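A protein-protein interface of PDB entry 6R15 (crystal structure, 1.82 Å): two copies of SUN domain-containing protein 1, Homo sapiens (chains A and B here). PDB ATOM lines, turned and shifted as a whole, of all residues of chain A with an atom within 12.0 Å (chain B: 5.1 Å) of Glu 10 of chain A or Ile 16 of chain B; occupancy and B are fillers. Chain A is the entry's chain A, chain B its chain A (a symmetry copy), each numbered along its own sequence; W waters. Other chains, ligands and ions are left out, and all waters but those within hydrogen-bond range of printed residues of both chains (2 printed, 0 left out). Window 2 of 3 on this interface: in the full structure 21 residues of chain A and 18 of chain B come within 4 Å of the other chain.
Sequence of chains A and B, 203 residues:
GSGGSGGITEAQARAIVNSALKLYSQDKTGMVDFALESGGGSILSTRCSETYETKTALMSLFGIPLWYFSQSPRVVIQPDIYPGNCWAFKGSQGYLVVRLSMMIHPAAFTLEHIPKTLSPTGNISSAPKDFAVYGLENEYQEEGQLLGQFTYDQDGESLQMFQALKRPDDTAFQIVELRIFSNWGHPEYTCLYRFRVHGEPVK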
ATOM      1  N   GLY A   6      -0.139 -11.825 -16.058  1.00  0.00           N
ATOM      2  CA  GLY A   6       0.437 -12.468 -17.226  1.00  0.00           C
ATOM      3  C   GLY A   6       1.800 -13.130 -17.028  1.00  0.00           C
ATOM      4  O   GLY A   6       2.146 -14.048 -17.778  1.00  0.00           O
ATOM      5  N   GLY A   7       2.565 -12.676 -16.014  1.00  0.00           N
ATOM      6  CA  GLY A   7       3.926 -13.126 -15.815  1.00  0.00           C
ATOM      7  C   GLY A   7       4.060 -14.215 -14.768  1.00  0.00           C
ATOM      8  O   GLY A   7       3.259 -14.317 -13.849  1.00  0.00           O
ATOM      9  N   ILE A   8       5.111 -14.997 -14.886  1.00  0.00           N
ATOM     10  CA  ILE A   8       5.316 -16.143 -14.004  1.00  0.00           C
ATOM     11  C   ILE A   8       6.250 -15.782 -12.853  1.00  0.00           C
ATOM     12  O   ILE A   8       7.119 -14.904 -12.977  1.00  0.00           O
ATOM     13  CB  ILE A   8       5.864 -17.357 -14.783  1.00  0.00           C
ATOM     14  CG1 ILE A   8       7.149 -17.019 -15.515  1.00  0.00           C
ATOM     15  CG2 ILE A   8       4.836 -17.839 -15.763  1.00  0.00           C
ATOM     16  CD1 ILE A   8       7.992 -18.253 -15.710  1.00  0.00           C
ATOM     17  N   THR A   9       6.093 -16.507 -11.739  1.00  0.00           N
ATOM     18  CA  THR A   9       6.949 -16.349 -10.576  1.00  0.00           C
ATOM     19  C   THR A   9       8.211 -17.213 -10.682  1.00  0.00           C
ATOM     20  O   THR A   9       8.312 -18.132 -11.509  1.00  0.00           O
ATOM     21  CB  THR A   9       6.209 -16.753  -9.297  1.00  0.00           C
ATOM     22  OG1 THR A   9       5.938 -18.160  -9.331  1.00  0.00           O
ATOM     23  CG2 THR A   9       4.888 -15.987  -9.149  1.00  0.00           C
ATOM     24  N   GLU A  10       9.160 -16.951  -9.767  1.00  0.00           N
ATOM     25  CA  GLU A  10      10.368 -17.769  -9.698  1.00  0.00           C
ATOM     26  C   GLU A  10      10.031 -19.227  -9.383  1.00  0.00           C
ATOM     27  O   GLU A  10      10.597 -20.146 -10.003  1.00  0.00           O
ATOM     28  CB  GLU A  10      11.344 -17.190  -8.657  1.00  0.00           C
ATOM     29  CG  GLU A  10      12.607 -18.049  -8.460  1.00  0.00           C
ATOM     30  CD  GLU A  10      13.610 -17.560  -7.362  1.00  0.00           C
ATOM     31  OE1 GLU A  10      13.613 -16.363  -6.964  1.00  0.00           O
ATOM     32  OE2 GLU A  10      14.413 -18.412  -6.925  1.00  0.00           O
ATOM     33  N   ALA A  11       9.085 -19.471  -8.456  1.00  0.00           N
ATOM     34  CA  ALA A  11       8.698 -20.859  -8.163  1.00  0.00           C
ATOM     35  C   ALA A  11       8.167 -21.575  -9.416  1.00  0.00           C
ATOM     36  O   ALA A  11       8.464 -22.754  -9.663  1.00  0.00           O
ATOM     37  CB  ALA A  11       7.649 -20.897  -7.045  1.00  0.00           C
ATOM     38  N   GLN A  12       7.332 -20.885 -10.193  1.00  0.00           N
ATOM     39  CA  GLN A  12       6.766 -21.492 -11.391  1.00  0.00           C
ATOM     40  C   GLN A  12       7.835 -21.757 -12.446  1.00  0.00           C
ATOM     41  O   GLN A  12       7.777 -22.777 -13.166  1.00  0.00           O
ATOM     42  CB  GLN A  12       5.675 -20.573 -11.938  1.00  0.00           C
ATOM     43  CG  GLN A  12       4.415 -20.567 -11.075  1.00  0.00           C
ATOM     44  CD  GLN A  12       3.427 -19.466 -11.451  1.00  0.00           C
ATOM     45  OE1 GLN A  12       3.791 -18.412 -11.974  1.00  0.00           O
ATOM     46  NE2 GLN A  12       2.172 -19.716 -11.174  1.00  0.00           N
ATOM     47  N   ALA A  13       8.809 -20.849 -12.588  1.00  0.00           N
ATOM     48  CA  ALA A  13       9.901 -21.062 -13.528  1.00  0.00           C
ATOM     49  C   ALA A  13      10.767 -22.254 -13.132  1.00  0.00           C
ATOM     50  O   ALA A  13      11.230 -23.040 -13.988  1.00  0.00           O
ATOM     51  CB  ALA A  13      10.770 -19.813 -13.599  1.00  0.00           C
ATOM     52  N   ARG A  14      11.021 -22.397 -11.818  1.00  0.00           N
ATOM     53  CA  ARG A  14      11.790 -23.550 -11.363  1.00  0.00           C
ATOM     54  C   ARG A  14      11.056 -24.854 -11.649  1.00  0.00           C
ATOM     55  O   ARG A  14      11.690 -25.841 -12.032  1.00  0.00           O
ATOM     56  CB  ARG A  14      12.096 -23.424  -9.862  1.00  0.00           C
ATOM     57  CG  ARG A  14      13.158 -22.349  -9.545  1.00  0.00           C
ATOM     58  CD  ARG A  14      13.368 -22.174  -8.015  1.00  0.00           C
ATOM     59  NE  ARG A  14      14.446 -21.227  -7.717  1.00  0.00           N
ATOM     60  CZ  ARG A  14      15.738 -21.556  -7.630  1.00  0.00           C
ATOM     61  NH1 ARG A  14      16.141 -22.813  -7.766  1.00  0.00           N
ATOM     62  NH2 ARG A  14      16.648 -20.620  -7.383  1.00  0.00           N
ATOM     63  N   ALA A  15       9.739 -24.891 -11.456  1.00  0.00           N
ATOM     64  CA  ALA A  15       8.972 -26.109 -11.739  1.00  0.00           C
ATOM     65  C   ALA A  15       9.033 -26.499 -13.227  1.00  0.00           C
ATOM     66  O   ALA A  15       9.187 -27.688 -13.557  1.00  0.00           O
ATOM     67  CB  ALA A  15       7.521 -25.927 -11.284  1.00  0.00           C
ATOM     68  N   ILE A  16       8.951 -25.517 -14.135  1.00  0.00           N
ATOM     69  CA  ILE A  16       9.040 -25.797 -15.576  1.00  0.00           C
ATOM     70  C   ILE A  16      10.423 -26.358 -15.959  1.00  0.00           C
ATOM     71  O   ILE A  16      10.528 -27.296 -16.765  1.00  0.00           O
ATOM     72  CB  ILE A  16       8.711 -24.517 -16.368  1.00  0.00           C
ATOM     73  CG1 ILE A  16       7.231 -24.173 -16.243  1.00  0.00           C
ATOM     74  CG2 ILE A  16       9.110 -24.622 -17.825  1.00  0.00           C
ATOM     75  CD1 ILE A  16       6.929 -22.787 -16.722  1.00  0.00           C
ATOM     76  N   VAL A  17      11.495 -25.780 -15.403  1.00  0.00           N
ATOM     77  CA  VAL A  17      12.854 -26.243 -15.680  1.00  0.00           C
ATOM     78  C   VAL A  17      13.050 -27.676 -15.181  1.00  0.00           C
ATOM     79  O   VAL A  17      13.583 -28.550 -15.901  1.00  0.00           O
ATOM     80  CB  VAL A  17      13.857 -25.273 -15.017  1.00  0.00           C
ATOM     81  CG1 VAL A  17      15.209 -25.809 -15.132  1.00  0.00           C
ATOM     82  CG2 VAL A  17      13.790 -23.870 -15.672  1.00  0.00           C
ATOM     83  N   ASN A  18      12.639 -27.939 -13.933  1.00  0.00           N
ATOM     84  CA  ASN A  18      12.831 -29.264 -13.342  1.00  0.00           C
ATOM     85  C   ASN A  18      12.030 -30.339 -14.088  1.00  0.00           C
ATOM     86  O   ASN A  18      12.508 -31.483 -14.235  1.00  0.00           O
ATOM     87  CB  ASN A  18      12.466 -29.247 -11.856  1.00  0.00           C
ATOM     88  CG  ASN A  18      13.438 -28.392 -11.010  1.00  0.00           C
ATOM     89  OD1 ASN A  18      14.578 -28.117 -11.401  1.00  0.00           O
ATOM     90  ND2 ASN A  18      12.961 -27.944  -9.861  1.00  0.00           N
ATOM     91  N   SER A  19      10.813 -29.998 -14.556  1.00  0.00           N
ATOM     92  CA  SER A  19      10.002 -30.955 -15.311  1.00  0.00           C
ATOM     93  C   SER A  19      10.641 -31.280 -16.664  1.00  0.00           C
ATOM     94  O   SER A  19      10.614 -32.440 -17.118  1.00  0.00           O
ATOM     95  CB  SER A  19       8.591 -30.408 -15.522  1.00  0.00           C
ATOM     96  OG  SER A  19       7.793 -30.546 -14.368  1.00  0.00           O
ATOM     97  N   ALA A  20      11.204 -30.273 -17.331  1.00  0.00           N
ATOM     98  CA  ALA A  20      11.887 -30.508 -18.610  1.00  0.00           C
ATOM     99  C   ALA A  20      13.134 -31.383 -18.466  1.00  0.00           C
ATOM    100  O   ALA A  20      13.390 -32.258 -19.327  1.00  0.00           O
ATOM    101  CB  ALA A  20      12.259 -29.160 -19.251  1.00  0.00           C
ATOM    102  N   LEU A  21      13.956 -31.155 -17.420  1.00  0.00           N
ATOM    103  CA  LEU A  21      15.124 -32.023 -17.198  1.00  0.00           C
ATOM    104  C   LEU A  21      14.711 -33.446 -16.812  1.00  0.00           C
ATOM    105  O   LEU A  21      15.384 -34.417 -17.202  1.00  0.00           O
ATOM    106  CB  LEU A  21      16.022 -31.430 -16.111  1.00  0.00           C
ATOM    107  CG  LEU A  21      16.979 -30.332 -16.569  1.00  0.00           C
ATOM    108  CD1 LEU A  21      17.708 -29.680 -15.353  1.00  0.00           C
ATOM    109  CD2 LEU A  21      17.981 -30.952 -17.496  1.00  0.00           C
ATOM    110  N   GLY B   6       6.244  -9.296  -8.526  1.00  0.00           N
ATOM    111  CA  GLY B   6       6.120 -10.733  -8.349  1.00  0.00           C
ATOM    112  C   GLY B   6       6.719 -11.602  -9.453  1.00  0.00           C
ATOM    113  O   GLY B   6       7.062 -12.760  -9.198  1.00  0.00           O
ATOM    114  N   ILE B   8       9.295 -12.660 -12.813  1.00  0.00           N
ATOM    115  CA  ILE B   8      10.724 -12.699 -13.105  1.00  0.00           C
ATOM    116  C   ILE B   8      11.005 -12.172 -14.510  1.00  0.00           C
ATOM    117  O   ILE B   8      10.162 -12.267 -15.416  1.00  0.00           O
ATOM    118  CB  ILE B   8      11.290 -14.124 -12.940  1.00  0.00           C
ATOM    119  CG1 ILE B   8      10.549 -15.125 -13.805  1.00  0.00           C
ATOM    120  CG2 ILE B   8      11.208 -14.541 -11.502  1.00  0.00           C
ATOM    121  CD1 ILE B   8      11.436 -16.294 -14.149  1.00  0.00           C
ATOM    122  N   GLN B  12      16.677 -13.330 -15.396  1.00  0.00           N
ATOM    123  CA  GLN B  12      16.558 -14.195 -14.230  1.00  0.00           C
ATOM    124  C   GLN B  12      16.155 -15.614 -14.620  1.00  0.00           C
ATOM    125  O   GLN B  12      16.620 -16.597 -14.004  1.00  0.00           O
ATOM    126  CB  GLN B  12      15.542 -13.584 -13.266  1.00  0.00           C
ATOM    127  CG  GLN B  12      16.065 -12.334 -12.564  1.00  0.00           C
ATOM    128  CD  GLN B  12      14.986 -11.564 -11.810  1.00  0.00           C
ATOM    129  OE1 GLN B  12      13.800 -11.602 -12.145  1.00  0.00           O
ATOM    130  NE2 GLN B  12      15.404 -10.858 -10.789  1.00  0.00           N
ATOM    131  N   ALA B  13      15.273 -15.759 -15.616  1.00  0.00           N
ATOM    132  CA  ALA B  13      14.888 -17.081 -16.089  1.00  0.00           C
ATOM    133  C   ALA B  13      16.061 -17.820 -16.727  1.00  0.00           C
ATOM    134  O   ALA B  13      16.231 -19.047 -16.556  1.00  0.00           O
ATOM    135  CB  ALA B  13      13.763 -16.955 -17.109  1.00  0.00           C
ATOM    136  N   ARG B  14      16.884 -17.083 -17.495  1.00  0.00           N
ATOM    137  CA  ARG B  14      18.062 -17.712 -18.083  1.00  0.00           C
ATOM    138  C   ARG B  14      19.033 -18.187 -17.008  1.00  0.00           C
ATOM    139  O   ARG B  14      19.621 -19.262 -17.147  1.00  0.00           O
ATOM    140  CB  ARG B  14      18.760 -16.736 -19.044  1.00  0.00           C
ATOM    141  CG  ARG B  14      17.983 -16.518 -20.359  1.00  0.00           C
ATOM    142  CD  ARG B  14      18.659 -15.449 -21.263  1.00  0.00           C
ATOM    143  NE  ARG B  14      17.979 -15.314 -22.553  1.00  0.00           N
ATOM    144  CZ  ARG B  14      18.241 -16.064 -23.628  1.00  0.00           C
ATOM    145  NH1 ARG B  14      19.201 -16.981 -23.613  1.00  0.00           N
ATOM    146  NH2 ARG B  14      17.549 -15.887 -24.748  1.00  0.00           N
ATOM    147  N   ALA B  15      19.230 -17.405 -15.948  1.00  0.00           N
ATOM    148  CA  ALA B  15      20.132 -17.818 -14.868  1.00  0.00           C
ATOM    149  C   ALA B  15      19.645 -19.099 -14.165  1.00  0.00           C
ATOM    150  O   ALA B  15      20.454 -19.995 -13.865  1.00  0.00           O
ATOM    151  CB  ALA B  15      20.295 -16.676 -13.861  1.00  0.00           C
ATOM    152  N   ILE B  16      18.331 -19.222 -13.928  1.00  0.00           N
ATOM    153  CA  ILE B  16      17.777 -20.429 -13.297  1.00  0.00           C
ATOM    154  C   ILE B  16      17.974 -21.673 -14.186  1.00  0.00           C
ATOM    155  O   ILE B  16      18.314 -22.759 -13.692  1.00  0.00           O
ATOM    156  CB  ILE B  16      16.289 -20.198 -12.970  1.00  0.00           C
ATOM    157  CG1 ILE B  16      16.139 -19.196 -11.830  1.00  0.00           C
ATOM    158  CG2 ILE B  16      15.565 -21.487 -12.641  1.00  0.00           C
ATOM    159  CD1 ILE B  16      14.732 -18.704 -11.691  1.00  0.00           C
ATOM    160  N   VAL B  17      17.742 -21.532 -15.497  1.00  0.00           N
ATOM    161  CA  VAL B  17      17.916 -22.640 -16.435  1.00  0.00           C
ATOM    162  C   VAL B  17      19.378 -23.087 -16.481  1.00  0.00           C
ATOM    163  O   VAL B  17      19.692 -24.297 -16.410  1.00  0.00           O
ATOM    164  CB  VAL B  17      17.418 -22.197 -17.828  1.00  0.00           C
ATOM    165  CG1 VAL B  17      17.741 -23.222 -18.816  1.00  0.00           C
ATOM    166  CG2 VAL B  17      15.889 -21.941 -17.818  1.00  0.00           C
ATOM    167  N   ASN B  18      20.297 -22.122 -16.617  1.00  0.00           N
ATOM    168  CA  ASN B  18      21.720 -22.448 -16.726  1.00  0.00           C
ATOM    169  C   ASN B  18      22.251 -23.104 -15.445  1.00  0.00           C
ATOM    170  O   ASN B  18      23.107 -24.011 -15.517  1.00  0.00           O
ATOM    171  CB  ASN B  18      22.532 -21.199 -17.075  1.00  0.00           C
ATOM    172  CG  ASN B  18      22.231 -20.667 -18.495  1.00  0.00           C
ATOM    173  OD1 ASN B  18      21.735 -21.384 -19.372  1.00  0.00           O
ATOM    174  ND2 ASN B  18      22.504 -19.390 -18.702  1.00  0.00           N
ATOM    175  N   SER B  19      21.767 -22.657 -14.269  1.00  0.00           N
ATOM    176  CA  SER B  19      22.195 -23.257 -13.003  1.00  0.00           C
ATOM    177  C   SER B  19      21.700 -24.700 -12.875  1.00  0.00           C
ATOM    178  O   SER B  19      22.426 -25.579 -12.371  1.00  0.00           O
ATOM    179  CB  SER B  19      21.688 -22.428 -11.824  1.00  0.00           C
ATOM    180  OG  SER B  19      22.470 -21.273 -11.614  1.00  0.00           O
ATOM    181  N   ALA B  20      20.468 -24.963 -13.307  1.00  0.00           N
ATOM    182  CA  ALA B  20      19.936 -26.331 -13.273  1.00  0.00           C
ATOM    183  C   ALA B  20      20.689 -27.286 -14.202  1.00  0.00           C
ATOM    184  O   ALA B  20      20.940 -28.457 -13.830  1.00  0.00           O
ATOM    185  CB  ALA B  20      18.441 -26.313 -13.634  1.00  0.00           C
HETATM  186  O   HOH W   1       7.219 -12.765 -15.083  1.00  0.00           O
HETATM  187  O   HOH W   2       8.993 -14.335  -8.364  1.00  0.00           O
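The backbone NH (N) of Ile 8 of chain B is in hydrogen-bond range of the backbone carbonyl oxygen (O) of Ile 8 of chain A (3.1 Å).
The guanidinium group (NE) of Arg 14 of chain A is in salt-bridge range of the side-chain carboxylate (OE2) of Glu 10 of chain A, at 2.9 Å. OE1 of Gln 12 of chain A lies within hydrogen-bond range of N of Thr 9 of chain A (3.0 Å).
Among the printed residues, merely in contact across the chains: Thr 9 of chain A with Gly 6 of chain B (3.8 Å), Glu 10 of chain A with Ile 8 of chain B (3.6 Å), Glu 10 of chain A with Ile 16 of chain B (3.9 Å), Ala 13 of chain A with Ile 8 of chain B (3.6 Å), Val 17 of chain A with Val 17 of chain B (3.6 Å), Val 17 of chain A with Ala 20 of chain B (3.6 Å) and Leu 21 of chain A with Ala 20 of chain B (3.8 Å).
Printed residues of chain B within 4 Å of Thr 9 of chain A: Gly 6 (3.8 Å). Glu 10 of chain A touches just these residues of chain B: Ile 8 and Ile 16. Of the printed residues of chain B, Ala 13 of chain A touches Ile 8 (3.6 Å). Of the printed residues of chain B, Val 17 of chain A touches Val 17 and Ala 20. Asn 18 of chain A touches none of the printed residues of chain B. Of the printed residues of chain B, Leu 21 of chain A touches Ala 20. Ile 8 of chain B touches three residues of chain A. No residue of chain A comes within 4 Å of Gln 12 of chain B. No residue of chain A comes within 4 Å of Ala 13 of chain B. Ala 15 of chain B touches none of the printed residues of chain A. Printed residues of chain A within 4 Å of Ile 16 of chain B: Glu 10 (3.9 Å). No residue of chain A comes within 4 Å of Asn 18 of chain B. The nearest residue of chain B that does not touch Glu 10 of chain A is Gly 6 of chain B (4.7 Å). The nearest printed residue of chain A that does not touch Ile 16 of chain B is Arg 14 of chain A (4.02 Å).
Among the printed residues, 8 pairs touch across the chains.
Ile 8 of chain B touches its own counterpart, Ile 8 of chain A. Ala 13 of chain A touches Ile 8 of chain B, but with the chains exchanged Ile 8 of chain A does not touch Ala 13 of chain B (6.1 Å). Val 17 of chain B touches its own counterpart, Val 17 of chain A. Val 17 of chain A touches Ala 20 of chain B, but with the chains exchanged Ala 20 of chain A does not touch Val 17 of chain B (8.1 Å). Of the 8 pairs that touch across the chains among the printed residues, 2 have their exchanged pair printed and touching as well.
Water W2 bridges the backbone carbonyl oxygen of Gly 6 of chain B (2.6 Å) and the backbone NH of Glu 10 of chain A (3.0 Å). Water W1 bridges the backbone carbonyl oxygen (O) of Ile 8 of chain A (3.0 Å) and the backbone carbonyl oxygen (O) of Ile 8 of chain B (3.0 Å).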
